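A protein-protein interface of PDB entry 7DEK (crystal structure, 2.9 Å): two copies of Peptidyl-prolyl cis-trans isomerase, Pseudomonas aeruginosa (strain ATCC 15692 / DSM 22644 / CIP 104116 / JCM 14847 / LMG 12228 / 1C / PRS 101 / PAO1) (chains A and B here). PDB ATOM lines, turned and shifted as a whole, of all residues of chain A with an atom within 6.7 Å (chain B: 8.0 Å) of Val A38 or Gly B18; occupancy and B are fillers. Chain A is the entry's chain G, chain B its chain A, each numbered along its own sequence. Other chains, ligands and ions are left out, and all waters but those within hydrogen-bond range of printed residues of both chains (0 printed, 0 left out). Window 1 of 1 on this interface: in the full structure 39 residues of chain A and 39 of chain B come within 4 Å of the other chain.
Ser A35 touches Ala B39, and with the chains exchanged Ala A39 touches Ser B35.
Ser A35 touches Ile B42, and with the chains exchanged Ile A42 touches Ser B35.
Val A38 touches Ile B42, and with the chains exchanged Ile A42 touches Val B38.
Ala B39 touches its own counterpart, Ala A39.
7 positions are printed for both chains.
Of the 31 pairs that touch across the chains among the printed residues, 10 have their exchanged pair printed and touching as well.
The side-chain hydroxyl of Ser B35 sits at hydrogen-bond distance from the backbone carbonyl oxygen of Ala A39, at 2.9 Å.
OD2 of Asp A34 sits at hydrogen-bond distance from NE2 of Gln B11.
OG of Ser B14 is in hydrogen-bond range of O of Ala B10 (2.8 Å).
The side-chain amino group of Lys B12 is in hydrogen-bond range of the backbone carbonyl oxygen of Leu B6 (3.0 Å).
The side-chain carboxylate of Asp A34 lies close to the backbone NH of Lys A36.
Ala A37 touches just these residues of chain B: Leu B6, Gln B11, Ser B14 and Tyr B15.
Of chain B, only Ser B14, Gly B18 and Ile B42 come within 4 Å of Val A38.
Printed residues of chain B within 4 Å of Ala A39: Ser B35 and Ala B39.
Printed residues of chain B within 4 Å of Ala A45: Leu B19 (3.2 Å) and Lys B23 (3.9 Å).
Ala B10 touches none of the printed residues of chain A.
Ala B13 touches none of the printed residues of chain A.
Of the printed residues of chain A, Ser B14 touches Leu A33, Asp A34, Ala A37 and Val A38.
Of the printed residues of chain A, Ser B35 touches Ala A39, Ile A42 and Glu A43.
Printed residues of chain A within 4 Å of Ile B42: Met A21 (3.9 Å), Leu A33 (3.9 Å), Ser A35 (3.7 Å) and Val A38 (3.7 Å).
The nearest residue of chain B that does not touch Val A38 is Tyr B15 (4.1 Å).
The nearest residue of chain A that does not touch Gly B18 is Ala A45 (4.7 Å).
The nearest printed residue of chain A that does not touch Met B21 is Ile A42 (4.01 Å).
Hydrophobic or aromatic side chains of chain B that line the printed part of chain A: Val B4, Leu B6, Tyr B15, Ile B17, Leu B19, Met B21, Leu B33, Val B38, Ala B39 and Ile B42.
Along chain B the printed residues that touch a printed residue of chain A span positions 4 to 42.
Of the 13 printed residues of chain A, 13 touch a printed residue of chain B.
Along chain A the printed residues that touch a printed residue of chain B span positions 21 to 45.
Among the printed residues, pairs that only touch across the chains: Ser A35 with Ala B39 (3.0 Å), Ala A37 with Gln B11 (3.1 Å), Ala A45 with Leu B19 (3.2 Å), Glu A43 with Ser B35 (3.2 Å), Lys A36 with Val B4 (3.4 Å), Gly A41 with Leu B19 (3.4 Å), Ile A42 with Ser B35 (3.4 Å), Ile A42 with Gly B18 (3.4 Å), Gly A41 with Tyr B15 (3.4 Å), Val A38 with Ser B14 (3.5 Å), Leu A33 with Ser B14 (3.5 Å), Ala A37 with Tyr B15 (3.5 Å), Ile A42 with Val B38 (3.5 Å), Ala A39 with Ala B39 (3.6 Å), Ala A37 with Leu B6 (3.6 Å), Met A21 with Met B21 (3.7 Å), Lys A40 with Val B4 (3.7 Å), Val A38 with Ile B42 (3.7 Å), Ile A42 with Leu B33 (3.7 Å), Ser A35 with Ile B42 (3.7 Å), Met A21 with Ile B42 (3.9 Å), Asp A34 with Ser B14 (3.9 Å), Ala A45 with Lys B23 (3.9 Å), Ile A42 with Leu B19 (3.9 Å), Ala A37 with Ser B14 (3.9 Å), Met A21 with Ile B17 (3.9 Å), Leu A33 with Ile B42 (3.9 Å), Gly A41 with Gly B18 (3.9 Å) and Val A38 with Gly B18 (3.9 Å).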
ATOM      1  N   MET A  21     -20.220 -14.039  -1.551  1.00  0.00           N
ATOM      2  CA  MET A  21     -19.902 -13.436  -0.230  1.00  0.00           C
ATOM      3  C   MET A  21     -18.640 -12.588  -0.363  1.00  0.00           C
ATOM      4  O   MET A  21     -18.648 -11.438   0.104  1.00  0.00           O
ATOM      5  CB  MET A  21     -19.660 -14.527   0.815  1.00  0.00           C
ATOM      6  CG  MET A  21     -19.395 -13.989   2.204  1.00  0.00           C
ATOM      7  SD  MET A  21     -19.009 -15.302   3.386  1.00  0.00           S
ATOM      8  CE  MET A  21     -17.716 -16.170   2.500  1.00  0.00           C
ATOM      9  N   LEU A  33      -9.786  -9.553   3.930  1.00  0.00           N
ATOM     10  CA  LEU A  33     -10.497 -10.835   4.161  1.00  0.00           C
ATOM     11  C   LEU A  33      -9.587 -11.973   3.701  1.00  0.00           C
ATOM     12  O   LEU A  33      -9.360 -12.092   2.487  1.00  0.00           O
ATOM     13  CB  LEU A  33     -11.800 -10.831   3.358  1.00  0.00           C
ATOM     14  CG  LEU A  33     -12.944 -11.645   3.955  1.00  0.00           C
ATOM     15  CD1 LEU A  33     -13.564 -10.908   5.132  1.00  0.00           C
ATOM     16  CD2 LEU A  33     -13.999 -11.933   2.900  1.00  0.00           C
ATOM     17  N   ASP A  34      -9.058 -12.750   4.646  1.00  0.00           N
ATOM     18  CA  ASP A  34      -8.211 -13.907   4.266  1.00  0.00           C
ATOM     19  C   ASP A  34      -9.075 -15.162   4.261  1.00  0.00           C
ATOM     20  O   ASP A  34      -9.703 -15.449   5.291  1.00  0.00           O
ATOM     21  CB  ASP A  34      -6.967 -14.032   5.145  1.00  0.00           C
ATOM     22  CG  ASP A  34      -5.989 -15.096   4.679  1.00  0.00           C
ATOM     23  OD1 ASP A  34      -6.064 -15.490   3.499  1.00  0.00           O
ATOM     24  OD2 ASP A  34      -5.156 -15.522   5.503  1.00  0.00           O
ATOM     25  N   SER A  35      -9.118 -15.843   3.121  1.00  0.00           N
ATOM     26  CA  SER A  35      -9.937 -17.068   2.983  1.00  0.00           C
ATOM     27  C   SER A  35      -9.467 -18.116   3.984  1.00  0.00           C
ATOM     28  O   SER A  35     -10.292 -18.945   4.386  1.00  0.00           O
ATOM     29  CB  SER A  35      -9.767 -17.595   1.604  1.00  0.00           C
ATOM     30  OG  SER A  35      -8.441 -18.065   1.418  1.00  0.00           O
ATOM     31  N   LYS A  36      -8.197 -18.061   4.379  1.00  0.00           N
ATOM     32  CA  LYS A  36      -7.646 -19.106   5.278  1.00  0.00           C
ATOM     33  C   LYS A  36      -8.436 -19.123   6.585  1.00  0.00           C
ATOM     34  O   LYS A  36      -8.864 -20.210   7.000  1.00  0.00           O
ATOM     35  CB  LYS A  36      -6.161 -18.847   5.538  1.00  0.00           C
ATOM     36  CG  LYS A  36      -5.276 -18.842   4.299  1.00  0.00           C
ATOM     37  CD  LYS A  36      -5.438 -20.077   3.442  1.00  0.00           C
ATOM     38  CE  LYS A  36      -4.526 -20.072   2.236  1.00  0.00           C
ATOM     39  NZ  LYS A  36      -4.642 -18.807   1.474  1.00  0.00           N
ATOM     40  N   ALA A  37      -8.598 -17.962   7.215  1.00  0.00           N
ATOM     41  CA  ALA A  37      -9.303 -17.900   8.511  1.00  0.00           C
ATOM     42  C   ALA A  37     -10.709 -18.473   8.352  1.00  0.00           C
ATOM     43  O   ALA A  37     -11.088 -19.342   9.152  1.00  0.00           O
ATOM     44  CB  ALA A  37      -9.361 -16.476   8.978  1.00  0.00           C
ATOM     45  N   VAL A  38     -11.442 -18.004   7.346  1.00  0.00           N
ATOM     46  CA  VAL A  38     -12.840 -18.474   7.151  1.00  0.00           C
ATOM     47  C   VAL A  38     -12.814 -19.977   6.879  1.00  0.00           C
ATOM     48  O   VAL A  38     -13.675 -20.667   7.424  1.00  0.00           O
ATOM     49  CB  VAL A  38     -13.562 -17.682   6.043  1.00  0.00           C
ATOM     50  CG1 VAL A  38     -12.770 -16.460   5.613  1.00  0.00           C
ATOM     51  CG2 VAL A  38     -13.940 -18.537   4.843  1.00  0.00           C
ATOM     52  N   ALA A  39     -11.817 -20.471   6.144  1.00  0.00           N
ATOM     53  CA  ALA A  39     -11.779 -21.908   5.787  1.00  0.00           C
ATOM     54  C   ALA A  39     -11.887 -22.750   7.057  1.00  0.00           C
ATOM     55  O   ALA A  39     -12.874 -23.491   7.197  1.00  0.00           O
ATOM     56  CB  ALA A  39     -10.505 -22.218   5.053  1.00  0.00           C
ATOM     57  N   LYS A  40     -10.888 -22.646   7.934  1.00  0.00           N
ATOM     58  CA  LYS A  40     -10.866 -23.481   9.161  1.00  0.00           C
ATOM     59  C   LYS A  40     -12.082 -23.151  10.022  1.00  0.00           C
ATOM     60  O   LYS A  40     -12.608 -24.064  10.659  1.00  0.00           O
ATOM     61  CB  LYS A  40      -9.558 -23.283   9.928  1.00  0.00           C
ATOM     62  CG  LYS A  40      -8.514 -24.365   9.699  1.00  0.00           C
ATOM     63  CD  LYS A  40      -8.816 -25.647  10.441  1.00  0.00           C
ATOM     64  CE  LYS A  40      -8.843 -25.459  11.942  1.00  0.00           C
ATOM     65  NZ  LYS A  40      -9.153 -26.724  12.646  1.00  0.00           N
ATOM     66  N   GLY A  41     -12.472 -21.877  10.058  1.00  0.00           N
ATOM     67  CA  GLY A  41     -13.656 -21.473  10.834  1.00  0.00           C
ATOM     68  C   GLY A  41     -14.856 -22.320  10.473  1.00  0.00           C
ATOM     69  O   GLY A  41     -15.509 -22.846  11.388  1.00  0.00           O
ATOM     70  N   ILE A  42     -15.130 -22.443   9.173  1.00  0.00           N
ATOM     71  CA  ILE A  42     -16.261 -23.292   8.706  1.00  0.00           C
ATOM     72  C   ILE A  42     -15.976 -24.717   9.167  1.00  0.00           C
ATOM     73  O   ILE A  42     -16.883 -25.319   9.739  1.00  0.00           O
ATOM     74  CB  ILE A  42     -16.415 -23.223   7.176  1.00  0.00           C
ATOM     75  CG1 ILE A  42     -16.431 -21.782   6.666  1.00  0.00           C
ATOM     76  CG2 ILE A  42     -17.652 -23.977   6.723  1.00  0.00           C
ATOM     77  CD1 ILE A  42     -16.317 -21.660   5.174  1.00  0.00           C
ATOM     78  N   GLU A  43     -14.758 -25.214   8.932  1.00  0.00           N
ATOM     79  CA  GLU A  43     -14.412 -26.618   9.283  1.00  0.00           C
ATOM     80  C   GLU A  43     -14.716 -26.873  10.761  1.00  0.00           C
ATOM     81  O   GLU A  43     -15.276 -27.937  11.073  1.00  0.00           O
ATOM     82  CB  GLU A  43     -12.936 -26.898   9.000  1.00  0.00           C
ATOM     83  CG  GLU A  43     -12.565 -26.804   7.534  1.00  0.00           C
ATOM     84  CD  GLU A  43     -11.087 -26.996   7.250  1.00  0.00           C
ATOM     85  OE1 GLU A  43     -10.402 -27.606   8.093  1.00  0.00           O
ATOM     86  OE2 GLU A  43     -10.623 -26.528   6.193  1.00  0.00           O
ATOM     87  N   ALA A  45     -16.853 -25.382  12.663  1.00  0.00           N
ATOM     88  CA  ALA A  45     -18.326 -25.422  12.803  1.00  0.00           C
ATOM     89  C   ALA A  45     -18.863 -26.729  12.224  1.00  0.00           C
ATOM     90  O   ALA A  45     -19.771 -27.316  12.837  1.00  0.00           O
ATOM     91  CB  ALA A  45     -18.922 -24.240  12.090  1.00  0.00           C
ATOM     92  N   VAL B   4      -3.810 -22.313  10.847  1.00  0.00           N
ATOM     93  CA  VAL B   4      -4.358 -20.999  10.383  1.00  0.00           C
ATOM     94  C   VAL B   4      -3.790 -19.861  11.237  1.00  0.00           C
ATOM     95  O   VAL B   4      -3.644 -20.057  12.459  1.00  0.00           O
ATOM     96  CB  VAL B   4      -5.895 -20.990  10.385  1.00  0.00           C
ATOM     97  CG1 VAL B   4      -6.456 -21.372   9.026  1.00  0.00           C
ATOM     98  CG2 VAL B   4      -6.462 -21.875  11.483  1.00  0.00           C
ATOM     99  N   LEU B   6      -5.087 -16.679  12.106  1.00  0.00           N
ATOM    100  CA  LEU B   6      -6.070 -16.193  13.113  1.00  0.00           C
ATOM    101  C   LEU B   6      -5.391 -15.169  14.023  1.00  0.00           C
ATOM    102  O   LEU B   6      -5.794 -15.082  15.185  1.00  0.00           O
ATOM    103  CB  LEU B   6      -6.631 -17.362  13.925  1.00  0.00           C
ATOM    104  CG  LEU B   6      -7.270 -18.485  13.115  1.00  0.00           C
ATOM    105  CD1 LEU B   6      -7.962 -19.472  14.040  1.00  0.00           C
ATOM    106  CD2 LEU B   6      -8.252 -17.925  12.105  1.00  0.00           C
ATOM    107  N   ALA B  10      -8.443  -8.795  11.544  1.00  0.00           N
ATOM    108  CA  ALA B  10      -9.213  -9.149  10.331  1.00  0.00           C
ATOM    109  C   ALA B  10      -9.356 -10.668  10.274  1.00  0.00           C
ATOM    110  O   ALA B  10     -10.449 -11.143   9.942  1.00  0.00           O
ATOM    111  CB  ALA B  10      -8.495  -8.636   9.115  1.00  0.00           C
ATOM    112  N   GLN B  11      -8.274 -11.388  10.575  1.00  0.00           N
ATOM    113  CA  GLN B  11      -8.291 -12.873  10.542  1.00  0.00           C
ATOM    114  C   GLN B  11      -9.289 -13.398  11.568  1.00  0.00           C
ATOM    115  O   GLN B  11     -10.068 -14.295  11.225  1.00  0.00           O
ATOM    116  CB  GLN B  11      -6.911 -13.409  10.912  1.00  0.00           C
ATOM    117  CG  GLN B  11      -5.893 -13.361   9.787  1.00  0.00           C
ATOM    118  CD  GLN B  11      -6.188 -14.400   8.738  1.00  0.00           C
ATOM    119  OE1 GLN B  11      -7.242 -14.386   8.117  1.00  0.00           O
ATOM    120  NE2 GLN B  11      -5.254 -15.311   8.530  1.00  0.00           N
ATOM    121  N   LYS B  12      -9.222 -12.884  12.794  1.00  0.00           N
ATOM    122  CA  LYS B  12     -10.156 -13.320  13.858  1.00  0.00           C
ATOM    123  C   LYS B  12     -11.583 -13.160  13.337  1.00  0.00           C
ATOM    124  O   LYS B  12     -12.360 -14.122  13.445  1.00  0.00           O
ATOM    125  CB  LYS B  12      -9.925 -12.495  15.123  1.00  0.00           C
ATOM    126  CG  LYS B  12      -8.496 -12.518  15.646  1.00  0.00           C
ATOM    127  CD  LYS B  12      -8.318 -11.780  16.952  1.00  0.00           C
ATOM    128  CE  LYS B  12      -6.875 -11.740  17.407  1.00  0.00           C
ATOM    129  NZ  LYS B  12      -6.256 -13.087  17.384  1.00  0.00           N
ATOM    130  N   ALA B  13     -11.899 -11.993  12.772  1.00  0.00           N
ATOM    131  CA  ALA B  13     -13.266 -11.722  12.266  1.00  0.00           C
ATOM    132  C   ALA B  13     -13.605 -12.672  11.115  1.00  0.00           C
ATOM    133  O   ALA B  13     -14.689 -13.271  11.151  1.00  0.00           O
ATOM    134  CB  ALA B  13     -13.370 -10.282  11.840  1.00  0.00           C
ATOM    135  N   SER B  14     -12.717 -12.773  10.124  1.00  0.00           N
ATOM    136  CA  SER B  14     -12.968 -13.644   8.948  1.00  0.00           C
ATOM    137  C   SER B  14     -13.253 -15.062   9.436  1.00  0.00           C
ATOM    138  O   SER B  14     -14.135 -15.717   8.861  1.00  0.00           O
ATOM    139  CB  SER B  14     -11.797 -13.621   8.005  1.00  0.00           C
ATOM    140  OG  SER B  14     -11.504 -12.296   7.591  1.00  0.00           O
ATOM    141  N   TYR B  15     -12.533 -15.504  10.467  1.00  0.00           N
ATOM    142  CA  TYR B  15     -12.737 -16.864  11.026  1.00  0.00           C
ATOM    143  C   TYR B  15     -14.206 -17.027  11.398  1.00  0.00           C
ATOM    144  O   TYR B  15     -14.834 -17.992  10.937  1.00  0.00           O
ATOM    145  CB  TYR B  15     -11.865 -17.050  12.268  1.00  0.00           C
ATOM    146  CG  TYR B  15     -12.146 -18.291  13.076  1.00  0.00           C
ATOM    147  CD1 TYR B  15     -11.507 -19.482  12.787  1.00  0.00           C
ATOM    148  CD2 TYR B  15     -13.036 -18.274  14.137  1.00  0.00           C
ATOM    149  CE1 TYR B  15     -11.752 -20.627  13.523  1.00  0.00           C
ATOM    150  CE2 TYR B  15     -13.302 -19.413  14.877  1.00  0.00           C
ATOM    151  CZ  TYR B  15     -12.657 -20.595  14.566  1.00  0.00           C
ATOM    152  OH  TYR B  15     -12.907 -21.726  15.284  1.00  0.00           O
ATOM    153  N   GLY B  16     -14.720 -16.128  12.238  1.00  0.00           N
ATOM    154  CA  GLY B  16     -16.103 -16.262  12.734  1.00  0.00           C
ATOM    155  C   GLY B  16     -17.141 -16.073  11.650  1.00  0.00           C
ATOM    156  O   GLY B  16     -18.250 -16.605  11.804  1.00  0.00           O
ATOM    157  N   ILE B  17     -16.805 -15.352  10.583  1.00  0.00           N
ATOM    158  CA  ILE B  17     -17.772 -15.267   9.455  1.00  0.00           C
ATOM    159  C   ILE B  17     -18.007 -16.704   8.997  1.00  0.00           C
ATOM    160  O   ILE B  17     -19.172 -17.119   8.939  1.00  0.00           O
ATOM    161  CB  ILE B  17     -17.227 -14.372   8.326  1.00  0.00           C
ATOM    162  CG1 ILE B  17     -17.022 -12.932   8.799  1.00  0.00           C
ATOM    163  CG2 ILE B  17     -18.128 -14.435   7.103  1.00  0.00           C
ATOM    164  CD1 ILE B  17     -16.453 -12.017   7.742  1.00  0.00           C
ATOM    165  N   GLY B  18     -16.929 -17.457   8.785  1.00  0.00           N
ATOM    166  CA  GLY B  18     -17.052 -18.858   8.351  1.00  0.00           C
ATOM    167  C   GLY B  18     -17.647 -19.738   9.434  1.00  0.00           C
ATOM    168  O   GLY B  18     -18.465 -20.608   9.103  1.00  0.00           O
ATOM    169  N   LEU B  19     -17.218 -19.549  10.680  1.00  0.00           N
ATOM    170  CA  LEU B  19     -17.747 -20.359  11.805  1.00  0.00           C
ATOM    171  C   LEU B  19     -19.270 -20.234  11.801  1.00  0.00           C
ATOM    172  O   LEU B  19     -19.948 -21.256  11.638  1.00  0.00           O
ATOM    173  CB  LEU B  19     -17.155 -19.827  13.112  1.00  0.00           C
ATOM    174  CG  LEU B  19     -17.610 -20.530  14.387  1.00  0.00           C
ATOM    175  CD1 LEU B  19     -16.818 -21.809  14.605  1.00  0.00           C
ATOM    176  CD2 LEU B  19     -17.454 -19.604  15.582  1.00  0.00           C
ATOM    177  N   ASN B  20     -19.778 -19.013  11.974  1.00  0.00           N
ATOM    178  CA  ASN B  20     -21.245 -18.809  12.047  1.00  0.00           C
ATOM    179  C   ASN B  20     -21.879 -19.301  10.746  1.00  0.00           C
ATOM    180  O   ASN B  20     -22.977 -19.861  10.812  1.00  0.00           O
ATOM    181  CB  ASN B  20     -21.597 -17.357  12.368  1.00  0.00           C
ATOM    182  CG  ASN B  20     -22.820 -17.228  13.249  1.00  0.00           C
ATOM    183  OD1 ASN B  20     -23.516 -18.210  13.501  1.00  0.00           O
ATOM    184  ND2 ASN B  20     -23.087 -16.024  13.726  1.00  0.00           N
ATOM    185  N   MET B  21     -21.205 -19.091   9.614  1.00  0.00           N
ATOM    186  CA  MET B  21     -21.761 -19.485   8.293  1.00  0.00           C
ATOM    187  C   MET B  21     -21.961 -21.001   8.258  1.00  0.00           C
ATOM    188  O   MET B  21     -23.033 -21.436   7.828  1.00  0.00           O
ATOM    189  CB  MET B  21     -20.846 -19.036   7.149  1.00  0.00           C
ATOM    190  CG  MET B  21     -20.503 -20.115   6.141  1.00  0.00           C
ATOM    191  SD  MET B  21     -19.623 -19.440   4.716  1.00  0.00           S
ATOM    192  CE  MET B  21     -20.900 -18.380   4.042  1.00  0.00           C
ATOM    193  N   GLY B  22     -20.984 -21.769   8.740  1.00  0.00           N
ATOM    194  CA  GLY B  22     -21.131 -23.234   8.784  1.00  0.00           C
ATOM    195  C   GLY B  22     -22.344 -23.626   9.603  1.00  0.00           C
ATOM    196  O   GLY B  22     -23.144 -24.436   9.116  1.00  0.00           O
ATOM    197  N   LYS B  23     -22.488 -23.037  10.788  1.00  0.00           N
ATOM    198  CA  LYS B  23     -23.633 -23.363  11.675  1.00  0.00           C
ATOM    199  C   LYS B  23     -24.933 -22.893  11.017  1.00  0.00           C
ATOM    200  O   LYS B  23     -25.923 -23.635  11.073  1.00  0.00           O
ATOM    201  CB  LYS B  23     -23.423 -22.723  13.050  1.00  0.00           C
ATOM    202  CG  LYS B  23     -22.224 -23.247  13.830  1.00  0.00           C
ATOM    203  CD  LYS B  23     -22.058 -22.610  15.194  1.00  0.00           C
ATOM    204  CE  LYS B  23     -21.806 -21.120  15.129  1.00  0.00           C
ATOM    205  NZ  LYS B  23     -21.611 -20.539  16.477  1.00  0.00           N
ATOM    206  N   SER B  24     -24.935 -21.696  10.431  1.00  0.00           N
ATOM    207  CA  SER B  24     -26.153 -21.162   9.771  1.00  0.00           C
ATOM    208  C   SER B  24     -26.569 -22.104   8.643  1.00  0.00           C
ATOM    209  O   SER B  24     -27.737 -22.520   8.623  1.00  0.00           O
ATOM    210  CB  SER B  24     -25.929 -19.772   9.254  1.00  0.00           C
ATOM    211  OG  SER B  24     -27.033 -19.346   8.469  1.00  0.00           O
ATOM    212  N   LEU B  25     -25.634 -22.450   7.759  1.00  0.00           N
ATOM    213  CA  LEU B  25     -25.969 -23.295   6.584  1.00  0.00           C
ATOM    214  C   LEU B  25     -26.321 -24.715   7.034  1.00  0.00           C
ATOM    215  O   LEU B  25     -27.118 -25.363   6.343  1.00  0.00           O
ATOM    216  CB  LEU B  25     -24.781 -23.288   5.621  1.00  0.00           C
ATOM    217  CG  LEU B  25     -24.497 -21.941   4.959  1.00  0.00           C
ATOM    218  CD1 LEU B  25     -23.289 -22.030   4.041  1.00  0.00           C
ATOM    219  CD2 LEU B  25     -25.714 -21.447   4.193  1.00  0.00           C
ATOM    220  N   LEU B  33     -21.753 -28.649   2.470  1.00  0.00           N
ATOM    221  CA  LEU B  33     -20.771 -27.554   2.227  1.00  0.00           C
ATOM    222  C   LEU B  33     -19.378 -27.971   2.707  1.00  0.00           C
ATOM    223  O   LEU B  33     -19.283 -28.458   3.848  1.00  0.00           O
ATOM    224  CB  LEU B  33     -21.242 -26.304   2.973  1.00  0.00           C
ATOM    225  CG  LEU B  33     -20.301 -25.102   2.907  1.00  0.00           C
ATOM    226  CD1 LEU B  33     -20.658 -24.203   1.735  1.00  0.00           C
ATOM    227  CD2 LEU B  33     -20.344 -24.315   4.206  1.00  0.00           C
ATOM    228  N   SER B  35     -15.211 -26.461   3.063  1.00  0.00           N
ATOM    229  CA  SER B  35     -14.395 -25.225   2.983  1.00  0.00           C
ATOM    230  C   SER B  35     -13.486 -25.309   1.763  1.00  0.00           C
ATOM    231  O   SER B  35     -12.765 -24.350   1.504  1.00  0.00           O
ATOM    232  CB  SER B  35     -13.587 -25.064   4.230  1.00  0.00           C
ATOM    233  OG  SER B  35     -14.399 -25.243   5.380  1.00  0.00           O
ATOM    234  N   VAL B  38     -15.396 -22.766  -0.813  1.00  0.00           N
ATOM    235  CA  VAL B  38     -15.890 -21.449  -0.312  1.00  0.00           C
ATOM    236  C   VAL B  38     -14.666 -20.599   0.019  1.00  0.00           C
ATOM    237  O   VAL B  38     -14.665 -19.406  -0.326  1.00  0.00           O
ATOM    238  CB  VAL B  38     -16.845 -21.586   0.890  1.00  0.00           C
ATOM    239  CG1 VAL B  38     -16.441 -22.716   1.816  1.00  0.00           C
ATOM    240  CG2 VAL B  38     -17.011 -20.286   1.659  1.00  0.00           C
ATOM    241  N   ALA B  39     -13.633 -21.221   0.589  1.00  0.00           N
ATOM    242  CA  ALA B  39     -12.385 -20.486   0.888  1.00  0.00           C
ATOM    243  C   ALA B  39     -11.717 -20.108  -0.431  1.00  0.00           C
ATOM    244  O   ALA B  39     -11.279 -18.961  -0.568  1.00  0.00           O
ATOM    245  CB  ALA B  39     -11.473 -21.332   1.726  1.00  0.00           C
ATOM    246  N   LYS B  40     -11.656 -21.051  -1.367  1.00  0.00           N
ATOM    247  CA  LYS B  40     -11.076 -20.732  -2.693  1.00  0.00           C
ATOM    248  C   LYS B  40     -11.794 -19.502  -3.249  1.00  0.00           C
ATOM    249  O   LYS B  40     -11.094 -18.571  -3.666  1.00  0.00           O
ATOM    250  CB  LYS B  40     -11.212 -21.934  -3.632  1.00  0.00           C
ATOM    251  CG  LYS B  40     -10.397 -21.856  -4.916  1.00  0.00           C
ATOM    252  CD  LYS B  40      -8.908 -21.741  -4.675  1.00  0.00           C
ATOM    253  CE  LYS B  40      -8.126 -21.396  -5.925  1.00  0.00           C
ATOM    254  NZ  LYS B  40      -8.388 -22.357  -7.021  1.00  0.00           N
ATOM    255  N   ILE B  42     -13.116 -16.954  -2.077  1.00  0.00           N
ATOM    256  CA  ILE B  42     -12.740 -15.625  -1.514  1.00  0.00           C
ATOM    257  C   ILE B  42     -11.497 -15.119  -2.249  1.00  0.00           C
ATOM    258  O   ILE B  42     -11.530 -13.979  -2.739  1.00  0.00           O
ATOM    259  CB  ILE B  42     -12.540 -15.717   0.008  1.00  0.00           C
ATOM    260  CG1 ILE B  42     -13.823 -16.180   0.699  1.00  0.00           C
ATOM    261  CG2 ILE B  42     -12.036 -14.399   0.574  1.00  0.00           C
ATOM    262  CD1 ILE B  42     -13.897 -15.815   2.157  1.00  0.00           C
